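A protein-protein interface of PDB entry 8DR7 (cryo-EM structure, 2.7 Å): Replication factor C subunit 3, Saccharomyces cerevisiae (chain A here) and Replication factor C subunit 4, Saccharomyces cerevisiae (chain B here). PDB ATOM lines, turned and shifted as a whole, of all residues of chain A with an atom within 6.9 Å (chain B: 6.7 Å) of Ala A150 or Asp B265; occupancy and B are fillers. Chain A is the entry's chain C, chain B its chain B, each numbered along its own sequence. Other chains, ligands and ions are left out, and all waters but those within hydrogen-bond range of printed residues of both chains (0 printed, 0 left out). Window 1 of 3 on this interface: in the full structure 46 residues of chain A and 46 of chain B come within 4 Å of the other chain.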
ATOM      1  N   LEU A  50      26.560  -5.351 -22.718  1.00  0.00           N
ATOM      2  CA  LEU A  50      27.318  -6.445 -23.322  1.00  0.00           C
ATOM      3  C   LEU A  50      27.472  -6.110 -24.802  1.00  0.00           C
ATOM      4  O   LEU A  50      26.539  -6.296 -25.589  1.00  0.00           O
ATOM      5  CB  LEU A  50      26.620  -7.787 -23.117  1.00  0.00           C
ATOM      6  CG  LEU A  50      27.299  -9.037 -23.696  1.00  0.00           C
ATOM      7  CD1 LEU A  50      26.890  -9.294 -25.141  1.00  0.00           C
ATOM      8  CD2 LEU A  50      28.812  -8.940 -23.584  1.00  0.00           C
ATOM      9  N   TYR A  52      28.744  -7.107 -28.092  1.00  0.00           N
ATOM     10  CA  TYR A  52      29.174  -8.285 -28.833  1.00  0.00           C
ATOM     11  C   TYR A  52      29.402  -7.901 -30.287  1.00  0.00           C
ATOM     12  O   TYR A  52      28.521  -7.312 -30.922  1.00  0.00           O
ATOM     13  CB  TYR A  52      28.132  -9.401 -28.735  1.00  0.00           C
ATOM     14  CG  TYR A  52      28.369 -10.550 -29.690  1.00  0.00           C
ATOM     15  CD1 TYR A  52      29.336 -11.510 -29.424  1.00  0.00           C
ATOM     16  CD2 TYR A  52      27.624 -10.675 -30.854  1.00  0.00           C
ATOM     17  CE1 TYR A  52      29.554 -12.561 -30.293  1.00  0.00           C
ATOM     18  CE2 TYR A  52      27.836 -11.722 -31.729  1.00  0.00           C
ATOM     19  CZ  TYR A  52      28.802 -12.662 -31.443  1.00  0.00           C
ATOM     20  OH  TYR A  52      29.016 -13.708 -32.312  1.00  0.00           O
ATOM     21  N   ASP A 120      35.569 -12.803 -22.926  1.00  0.00           N
ATOM     22  CA  ASP A 120      35.398 -14.164 -23.425  1.00  0.00           C
ATOM     23  C   ASP A 120      36.577 -15.064 -23.084  1.00  0.00           C
ATOM     24  O   ASP A 120      36.456 -16.286 -23.212  1.00  0.00           O
ATOM     25  CB  ASP A 120      35.185 -14.164 -24.943  1.00  0.00           C
ATOM     26  CG  ASP A 120      36.007 -13.103 -25.655  1.00  0.00           C
ATOM     27  OD1 ASP A 120      37.076 -12.728 -25.131  1.00  0.00           O
ATOM     28  OD2 ASP A 120      35.581 -12.647 -26.736  1.00  0.00           O
ATOM     29  N   ALA A 147      32.834  -8.516 -26.033  1.00  0.00           N
ATOM     30  CA  ALA A 147      33.063  -9.882 -26.476  1.00  0.00           C
ATOM     31  C   ALA A 147      33.043  -9.972 -27.996  1.00  0.00           C
ATOM     32  O   ALA A 147      32.378  -9.188 -28.682  1.00  0.00           O
ATOM     33  CB  ALA A 147      32.013 -10.839 -25.893  1.00  0.00           C
ATOM     34  N   ASN A 148      33.792 -10.949 -28.508  1.00  0.00           N
ATOM     35  CA  ASN A 148      33.770 -11.324 -29.915  1.00  0.00           C
ATOM     36  C   ASN A 148      33.115 -12.672 -30.161  1.00  0.00           C
ATOM     37  O   ASN A 148      32.588 -12.897 -31.252  1.00  0.00           O
ATOM     38  CB  ASN A 148      35.196 -11.362 -30.480  1.00  0.00           C
ATOM     39  CG  ASN A 148      35.817  -9.984 -30.594  1.00  0.00           C
ATOM     40  OD1 ASN A 148      36.765  -9.657 -29.881  1.00  0.00           O
ATOM     41  ND2 ASN A 148      35.288  -9.171 -31.500  1.00  0.00           N
ATOM     42  N   TYR A 149      33.138 -13.568 -29.175  1.00  0.00           N
ATOM     43  CA  TYR A 149      32.512 -14.881 -29.277  1.00  0.00           C
ATOM     44  C   TYR A 149      31.575 -15.058 -28.093  1.00  0.00           C
ATOM     45  O   TYR A 149      32.022 -15.062 -26.941  1.00  0.00           O
ATOM     46  CB  TYR A 149      33.565 -15.993 -29.302  1.00  0.00           C
ATOM     47  CG  TYR A 149      34.784 -15.658 -30.132  1.00  0.00           C
ATOM     48  CD1 TYR A 149      34.685 -15.483 -31.505  1.00  0.00           C
ATOM     49  CD2 TYR A 149      36.032 -15.518 -29.541  1.00  0.00           C
ATOM     50  CE1 TYR A 149      35.797 -15.176 -32.267  1.00  0.00           C
ATOM     51  CE2 TYR A 149      37.149 -15.211 -30.295  1.00  0.00           C
ATOM     52  CZ  TYR A 149      37.025 -15.041 -31.657  1.00  0.00           C
ATOM     53  OH  TYR A 149      38.134 -14.736 -32.412  1.00  0.00           O
ATOM     54  N   ALA A 150      30.280 -15.203 -28.375  1.00  0.00           N
ATOM     55  CA  ALA A 150      29.285 -15.313 -27.315  1.00  0.00           C
ATOM     56  C   ALA A 150      29.265 -16.685 -26.656  1.00  0.00           C
ATOM     57  O   ALA A 150      28.778 -16.805 -25.527  1.00  0.00           O
ATOM     58  CB  ALA A 150      27.894 -14.996 -27.869  1.00  0.00           C
ATOM     59  N   HIS A 151      29.781 -17.719 -27.326  1.00  0.00           N
ATOM     60  CA  HIS A 151      29.741 -19.061 -26.757  1.00  0.00           C
ATOM     61  C   HIS A 151      30.657 -19.209 -25.550  1.00  0.00           C
ATOM     62  O   HIS A 151      30.507 -20.171 -24.789  1.00  0.00           O
ATOM     63  CB  HIS A 151      30.113 -20.095 -27.822  1.00  0.00           C
ATOM     64  CG  HIS A 151      31.580 -20.165 -28.112  1.00  0.00           C
ATOM     65  ND1 HIS A 151      32.234 -19.220 -28.874  1.00  0.00           N
ATOM     66  CD2 HIS A 151      32.519 -21.069 -27.747  1.00  0.00           C
ATOM     67  CE1 HIS A 151      33.512 -19.539 -28.963  1.00  0.00           C
ATOM     68  NE2 HIS A 151      33.712 -20.656 -28.288  1.00  0.00           N
ATOM     69  N   LYS A 152      31.599 -18.286 -25.354  1.00  0.00           N
ATOM     70  CA  LYS A 152      32.500 -18.346 -24.210  1.00  0.00           C
ATOM     71  C   LYS A 152      31.899 -17.743 -22.947  1.00  0.00           C
ATOM     72  O   LYS A 152      32.511 -17.856 -21.878  1.00  0.00           O
ATOM     73  CB  LYS A 152      33.813 -17.630 -24.536  1.00  0.00           C
ATOM     74  CG  LYS A 152      34.555 -18.201 -25.736  1.00  0.00           C
ATOM     75  CD  LYS A 152      35.366 -19.437 -25.356  1.00  0.00           C
ATOM     76  CE  LYS A 152      36.870 -19.244 -25.543  1.00  0.00           C
ATOM     77  NZ  LYS A 152      37.239 -18.531 -26.801  1.00  0.00           N
ATOM     78  N   LEU A 153      30.732 -17.112 -23.037  1.00  0.00           N
ATOM     79  CA  LEU A 153      30.091 -16.477 -21.895  1.00  0.00           C
ATOM     80  C   LEU A 153      29.006 -17.386 -21.333  1.00  0.00           C
ATOM     81  O   LEU A 153      28.203 -17.951 -22.082  1.00  0.00           O
ATOM     82  CB  LEU A 153      29.487 -15.129 -22.292  1.00  0.00           C
ATOM     83  CG  LEU A 153      30.443 -14.130 -22.949  1.00  0.00           C
ATOM     84  CD1 LEU A 153      29.743 -12.802 -23.188  1.00  0.00           C
ATOM     85  CD2 LEU A 153      31.694 -13.932 -22.105  1.00  0.00           C
ATOM     86  N   THR A 154      28.988 -17.522 -20.010  1.00  0.00           N
ATOM     87  CA  THR A 154      28.002 -18.372 -19.365  1.00  0.00           C
ATOM     88  C   THR A 154      26.601 -17.783 -19.537  1.00  0.00           C
ATOM     89  O   THR A 154      26.435 -16.562 -19.595  1.00  0.00           O
ATOM     90  CB  THR A 154      28.315 -18.527 -17.879  1.00  0.00           C
ATOM     91  OG1 THR A 154      28.326 -17.238 -17.251  1.00  0.00           O
ATOM     92  CG2 THR A 154      29.667 -19.200 -17.681  1.00  0.00           C
ATOM     93  N   LEU A 158      25.146 -13.799 -19.332  1.00  0.00           N
ATOM     94  CA  LEU A 158      24.405 -13.197 -20.433  1.00  0.00           C
ATOM     95  C   LEU A 158      23.041 -12.690 -19.981  1.00  0.00           C
ATOM     96  O   LEU A 158      22.570 -11.658 -20.472  1.00  0.00           O
ATOM     97  CB  LEU A 158      24.239 -14.207 -21.568  1.00  0.00           C
ATOM     98  CG  LEU A 158      25.530 -14.666 -22.248  1.00  0.00           C
ATOM     99  CD1 LEU A 158      25.288 -15.923 -23.069  1.00  0.00           C
ATOM    100  CD2 LEU A 158      26.101 -13.560 -23.120  1.00  0.00           C
ATOM    101  N   ARG A 163      22.161  -6.707 -24.254  1.00  0.00           N
ATOM    102  CA  ARG A 163      23.003  -7.058 -25.390  1.00  0.00           C
ATOM    103  C   ARG A 163      22.929  -5.983 -26.467  1.00  0.00           C
ATOM    104  O   ARG A 163      21.837  -5.546 -26.845  1.00  0.00           O
ATOM    105  CB  ARG A 163      22.574  -8.406 -25.971  1.00  0.00           C
ATOM    106  CG  ARG A 163      23.723  -9.258 -26.475  1.00  0.00           C
ATOM    107  CD  ARG A 163      23.227 -10.517 -27.164  1.00  0.00           C
ATOM    108  NE  ARG A 163      23.061 -10.321 -28.601  1.00  0.00           N
ATOM    109  CZ  ARG A 163      23.711 -10.991 -29.545  1.00  0.00           C
ATOM    110  NH1 ARG A 163      24.602 -11.927 -29.250  1.00  0.00           N
ATOM    111  NH2 ARG A 163      23.462 -10.716 -30.823  1.00  0.00           N
ATOM    112  N   HIS B 232      19.678 -16.382 -32.334  1.00  0.00           N
ATOM    113  CA  HIS B 232      20.344 -17.019 -33.463  1.00  0.00           C
ATOM    114  C   HIS B 232      20.120 -18.531 -33.518  1.00  0.00           C
ATOM    115  O   HIS B 232      20.245 -19.112 -34.604  1.00  0.00           O
ATOM    116  CB  HIS B 232      21.847 -16.696 -33.473  1.00  0.00           C
ATOM    117  CG  HIS B 232      22.599 -17.180 -32.272  1.00  0.00           C
ATOM    118  ND1 HIS B 232      22.317 -16.755 -30.992  1.00  0.00           N
ATOM    119  CD2 HIS B 232      23.633 -18.048 -32.161  1.00  0.00           C
ATOM    120  CE1 HIS B 232      23.141 -17.344 -30.144  1.00  0.00           C
ATOM    121  NE2 HIS B 232      23.950 -18.133 -30.827  1.00  0.00           N
ATOM    122  N   VAL B 236      19.612 -20.601 -36.994  1.00  0.00           N
ATOM    123  CA  VAL B 236      20.432 -21.762 -37.326  1.00  0.00           C
ATOM    124  C   VAL B 236      19.550 -22.962 -37.638  1.00  0.00           C
ATOM    125  O   VAL B 236      19.804 -23.708 -38.592  1.00  0.00           O
ATOM    126  CB  VAL B 236      21.415 -22.060 -36.179  1.00  0.00           C
ATOM    127  CG1 VAL B 236      21.955 -23.477 -36.286  1.00  0.00           C
ATOM    128  CG2 VAL B 236      22.549 -21.049 -36.182  1.00  0.00           C
ATOM    129  N   GLY B 260      27.545 -10.091 -38.335  1.00  0.00           N
ATOM    130  CA  GLY B 260      28.654 -10.027 -37.407  1.00  0.00           C
ATOM    131  C   GLY B 260      28.879 -11.271 -36.575  1.00  0.00           C
ATOM    132  O   GLY B 260      29.851 -11.312 -35.811  1.00  0.00           O
ATOM    133  N   TYR B 261      28.023 -12.282 -36.694  1.00  0.00           N
ATOM    134  CA  TYR B 261      28.201 -13.501 -35.917  1.00  0.00           C
ATOM    135  C   TYR B 261      29.457 -14.239 -36.363  1.00  0.00           C
ATOM    136  O   TYR B 261      29.749 -14.340 -37.558  1.00  0.00           O
ATOM    137  CB  TYR B 261      26.978 -14.406 -36.063  1.00  0.00           C
ATOM    138  CG  TYR B 261      25.741 -13.871 -35.381  1.00  0.00           C
ATOM    139  CD1 TYR B 261      25.533 -14.068 -34.023  1.00  0.00           C
ATOM    140  CD2 TYR B 261      24.782 -13.164 -36.093  1.00  0.00           C
ATOM    141  CE1 TYR B 261      24.405 -13.580 -33.393  1.00  0.00           C
ATOM    142  CE2 TYR B 261      23.649 -12.672 -35.472  1.00  0.00           C
ATOM    143  CZ  TYR B 261      23.466 -12.882 -34.122  1.00  0.00           C
ATOM    144  OH  TYR B 261      22.341 -12.394 -33.499  1.00  0.00           O
ATOM    145  N   SER B 262      30.203 -14.755 -35.390  1.00  0.00           N
ATOM    146  CA  SER B 262      31.444 -15.454 -35.677  1.00  0.00           C
ATOM    147  C   SER B 262      31.167 -16.882 -36.143  1.00  0.00           C
ATOM    148  O   SER B 262      30.123 -17.470 -35.852  1.00  0.00           O
ATOM    149  CB  SER B 262      32.347 -15.472 -34.443  1.00  0.00           C
ATOM    150  OG  SER B 262      31.822 -16.322 -33.439  1.00  0.00           O
ATOM    151  N   SER B 263      32.132 -17.438 -36.879  1.00  0.00           N
ATOM    152  CA  SER B 263      31.985 -18.794 -37.394  1.00  0.00           C
ATOM    153  C   SER B 263      31.939 -19.817 -36.265  1.00  0.00           C
ATOM    154  O   SER B 263      31.180 -20.792 -36.334  1.00  0.00           O
ATOM    155  CB  SER B 263      33.128 -19.114 -38.357  1.00  0.00           C
ATOM    156  OG  SER B 263      34.376 -19.112 -37.687  1.00  0.00           O
ATOM    157  N   ILE B 264      32.751 -19.623 -35.224  1.00  0.00           N
ATOM    158  CA  ILE B 264      32.771 -20.570 -34.112  1.00  0.00           C
ATOM    159  C   ILE B 264      31.412 -20.605 -33.423  1.00  0.00           C
ATOM    160  O   ILE B 264      30.888 -21.680 -33.097  1.00  0.00           O
ATOM    161  CB  ILE B 264      33.905 -20.214 -33.128  1.00  0.00           C
ATOM    162  CG1 ILE B 264      33.950 -21.208 -31.965  1.00  0.00           C
ATOM    163  CG2 ILE B 264      33.742 -18.796 -32.588  1.00  0.00           C
ATOM    164  CD1 ILE B 264      34.319 -22.615 -32.377  1.00  0.00           C
ATOM    165  N   ASP B 265      30.814 -19.434 -33.195  1.00  0.00           N
ATOM    166  CA  ASP B 265      29.484 -19.393 -32.599  1.00  0.00           C
ATOM    167  C   ASP B 265      28.467 -20.086 -33.495  1.00  0.00           C
ATOM    168  O   ASP B 265      27.600 -20.822 -33.010  1.00  0.00           O
ATOM    169  CB  ASP B 265      29.071 -17.945 -32.342  1.00  0.00           C
ATOM    170  CG  ASP B 265      29.854 -17.305 -31.214  1.00  0.00           C
ATOM    171  OD1 ASP B 265      29.918 -17.901 -30.118  1.00  0.00           O
ATOM    172  OD2 ASP B 265      30.404 -16.204 -31.423  1.00  0.00           O
ATOM    173  N   ILE B 266      28.560 -19.864 -34.807  1.00  0.00           N
ATOM    174  CA  ILE B 266      27.608 -20.467 -35.736  1.00  0.00           C
ATOM    175  C   ILE B 266      27.708 -21.987 -35.684  1.00  0.00           C
ATOM    176  O   ILE B 266      26.694 -22.691 -35.624  1.00  0.00           O
ATOM    177  CB  ILE B 266      27.845 -19.937 -37.162  1.00  0.00           C
ATOM    178  CG1 ILE B 266      27.385 -18.481 -37.269  1.00  0.00           C
ATOM    179  CG2 ILE B 266      27.113 -20.803 -38.180  1.00  0.00           C
ATOM    180  CD1 ILE B 266      27.929 -17.754 -38.481  1.00  0.00           C
ATOM    181  N   VAL B 267      28.933 -22.516 -35.703  1.00  0.00           N
ATOM    182  CA  VAL B 267      29.101 -23.966 -35.718  1.00  0.00           C
ATOM    183  C   VAL B 267      28.669 -24.569 -34.387  1.00  0.00           C
ATOM    184  O   VAL B 267      28.069 -25.649 -34.349  1.00  0.00           O
ATOM    185  CB  VAL B 267      30.551 -24.343 -36.083  1.00  0.00           C
ATOM    186  CG1 VAL B 267      31.511 -24.039 -34.944  1.00  0.00           C
ATOM    187  CG2 VAL B 267      30.634 -25.811 -36.474  1.00  0.00           C
ATOM    188  N   THR B 268      28.953 -23.888 -33.272  1.00  0.00           N
ATOM    189  CA  THR B 268      28.503 -24.392 -31.978  1.00  0.00           C
ATOM    190  C   THR B 268      26.980 -24.420 -31.898  1.00  0.00           C
ATOM    191  O   THR B 268      26.387 -25.398 -31.417  1.00  0.00           O
ATOM    192  CB  THR B 268      29.085 -23.537 -30.853  1.00  0.00           C
ATOM    193  OG1 THR B 268      30.438 -23.183 -31.167  1.00  0.00           O
ATOM    194  CG2 THR B 268      29.060 -24.298 -29.538  1.00  0.00           C
ATOM    195  N   THR B 269      26.326 -23.355 -32.369  1.00  0.00           N
ATOM    196  CA  THR B 269      24.869 -23.317 -32.359  1.00  0.00           C
ATOM    197  C   THR B 269      24.289 -24.399 -33.260  1.00  0.00           C
ATOM    198  O   THR B 269      23.275 -25.021 -32.922  1.00  0.00           O
ATOM    199  CB  THR B 269      24.376 -21.937 -32.794  1.00  0.00           C
ATOM    200  OG1 THR B 269      25.102 -20.922 -32.088  1.00  0.00           O
ATOM    201  CG2 THR B 269      22.891 -21.784 -32.507  1.00  0.00           C
ATOM    202  N   SER B 270      24.912 -24.631 -34.417  1.00  0.00           N
ATOM    203  CA  SER B 270      24.471 -25.714 -35.289  1.00  0.00           C
ATOM    204  C   SER B 270      24.608 -27.061 -34.594  1.00  0.00           C
ATOM    205  O   SER B 270      23.722 -27.918 -34.699  1.00  0.00           O
ATOM    206  CB  SER B 270      25.272 -25.699 -36.590  1.00  0.00           C
ATOM    207  OG  SER B 270      25.123 -24.463 -37.267  1.00  0.00           O
ATOM    208  N   ARG B 272      24.463 -27.660 -31.346  1.00  0.00           N
ATOM    209  CA  ARG B 272      23.398 -27.787 -30.352  1.00  0.00           C
ATOM    210  C   ARG B 272      22.049 -28.057 -31.013  1.00  0.00           C
ATOM    211  O   ARG B 272      21.291 -28.933 -30.572  1.00  0.00           O
ATOM    212  CB  ARG B 272      23.322 -26.527 -29.488  1.00  0.00           C
ATOM    213  CG  ARG B 272      24.415 -26.422 -28.436  1.00  0.00           C
ATOM    214  CD  ARG B 272      25.108 -25.070 -28.481  1.00  0.00           C
ATOM    215  NE  ARG B 272      26.333 -25.056 -27.688  1.00  0.00           N
ATOM    216  CZ  ARG B 272      26.752 -24.032 -26.955  1.00  0.00           C
ATOM    217  NH1 ARG B 272      26.069 -22.900 -26.884  1.00  0.00           N
ATOM    218  NH2 ARG B 272      27.892 -24.143 -26.279  1.00  0.00           N
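The side-chain hydroxyl (OH) of Tyr B261 lies within hydrogen-bond range of the guanidinium group (NH2) of Arg A163 (3.4 Å). OH of Tyr A52 sits at hydrogen-bond distance from N of Ser B262 (3.5 Å). The side-chain carboxylate (OD2) of Asp B265 sits at hydrogen-bond distance from the side-chain hydroxyl (OH) of Tyr A52, at 3.0 Å. The backbone NH (N) of Ala A150 sits at hydrogen-bond distance from the side-chain carboxylate (OD2) of Asp B265 (3.2 Å). N of His A151 is in hydrogen-bond range of OD1 of Asp B265 (2.8 Å).
The side-chain hydroxyl (OG) of Ser B262 lies within hydrogen-bond range of the side-chain carboxylate (OD2) of Asp B265, 2.5 Å away. O of Ile B264 lies within hydrogen-bond range of OG1 of Thr B268 (2.5 Å). The backbone carbonyl oxygen (O) of Asp B265 is in hydrogen-bond range of the side-chain hydroxyl (OG1) of Thr B269, at 2.7 Å. The backbone NH (N) of Asn A148 is in hydrogen-bond range of the side-chain carboxylate (OD2) of Asp A120 (3.0 Å).
Tyr A52 touches Tyr B261 (OH to CA, 3.7 Å). Asp B265 touches Asn A148 (OD2 to O, 3.97 Å). Tyr A149 touches Ser B262 (CD1 to OG, 3.6 Å). Tyr A149 touches Ile B264 (CD1 to CG2, 3.6 Å). OD2 of Asp B265 touches CA of Tyr A149, at 3.3 Å. Ile B264 touches His A151.
Of chain B, only Asp B265 (3.2 Å) comes within 4 Å of Ala A150. Asp B265 touches just these residues of chain A: Tyr A52 (3.0 Å), Asn A148 (3.97 Å), Tyr A149 (3.3 Å), Ala A150 (3.2 Å) and His A151 (2.8 Å). Of the printed residues of chain B, Tyr A52 touches Tyr B261, Ser B262 and Asp B265. Of the printed residues of chain A, Ile B264 touches Tyr A149 and His A151. The nearest residue of chain B that does not touch Ala A150 is Ser B262 (5.4 Å).
Of the 13 printed residues of chain A, 6 touch a printed residue of chain B. Printed residues of chain A that touch a printed residue of chain B: Tyr A52, Asn A148, Tyr A149, Ala A150, His A151 and Arg A163. Of the 14 printed residues of chain B, 4 touch a printed residue of chain A. Among the printed residues, no Asp or Glu carboxylate lies within 4 Å of a Lys or Arg side-chain nitrogen of the other chain.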
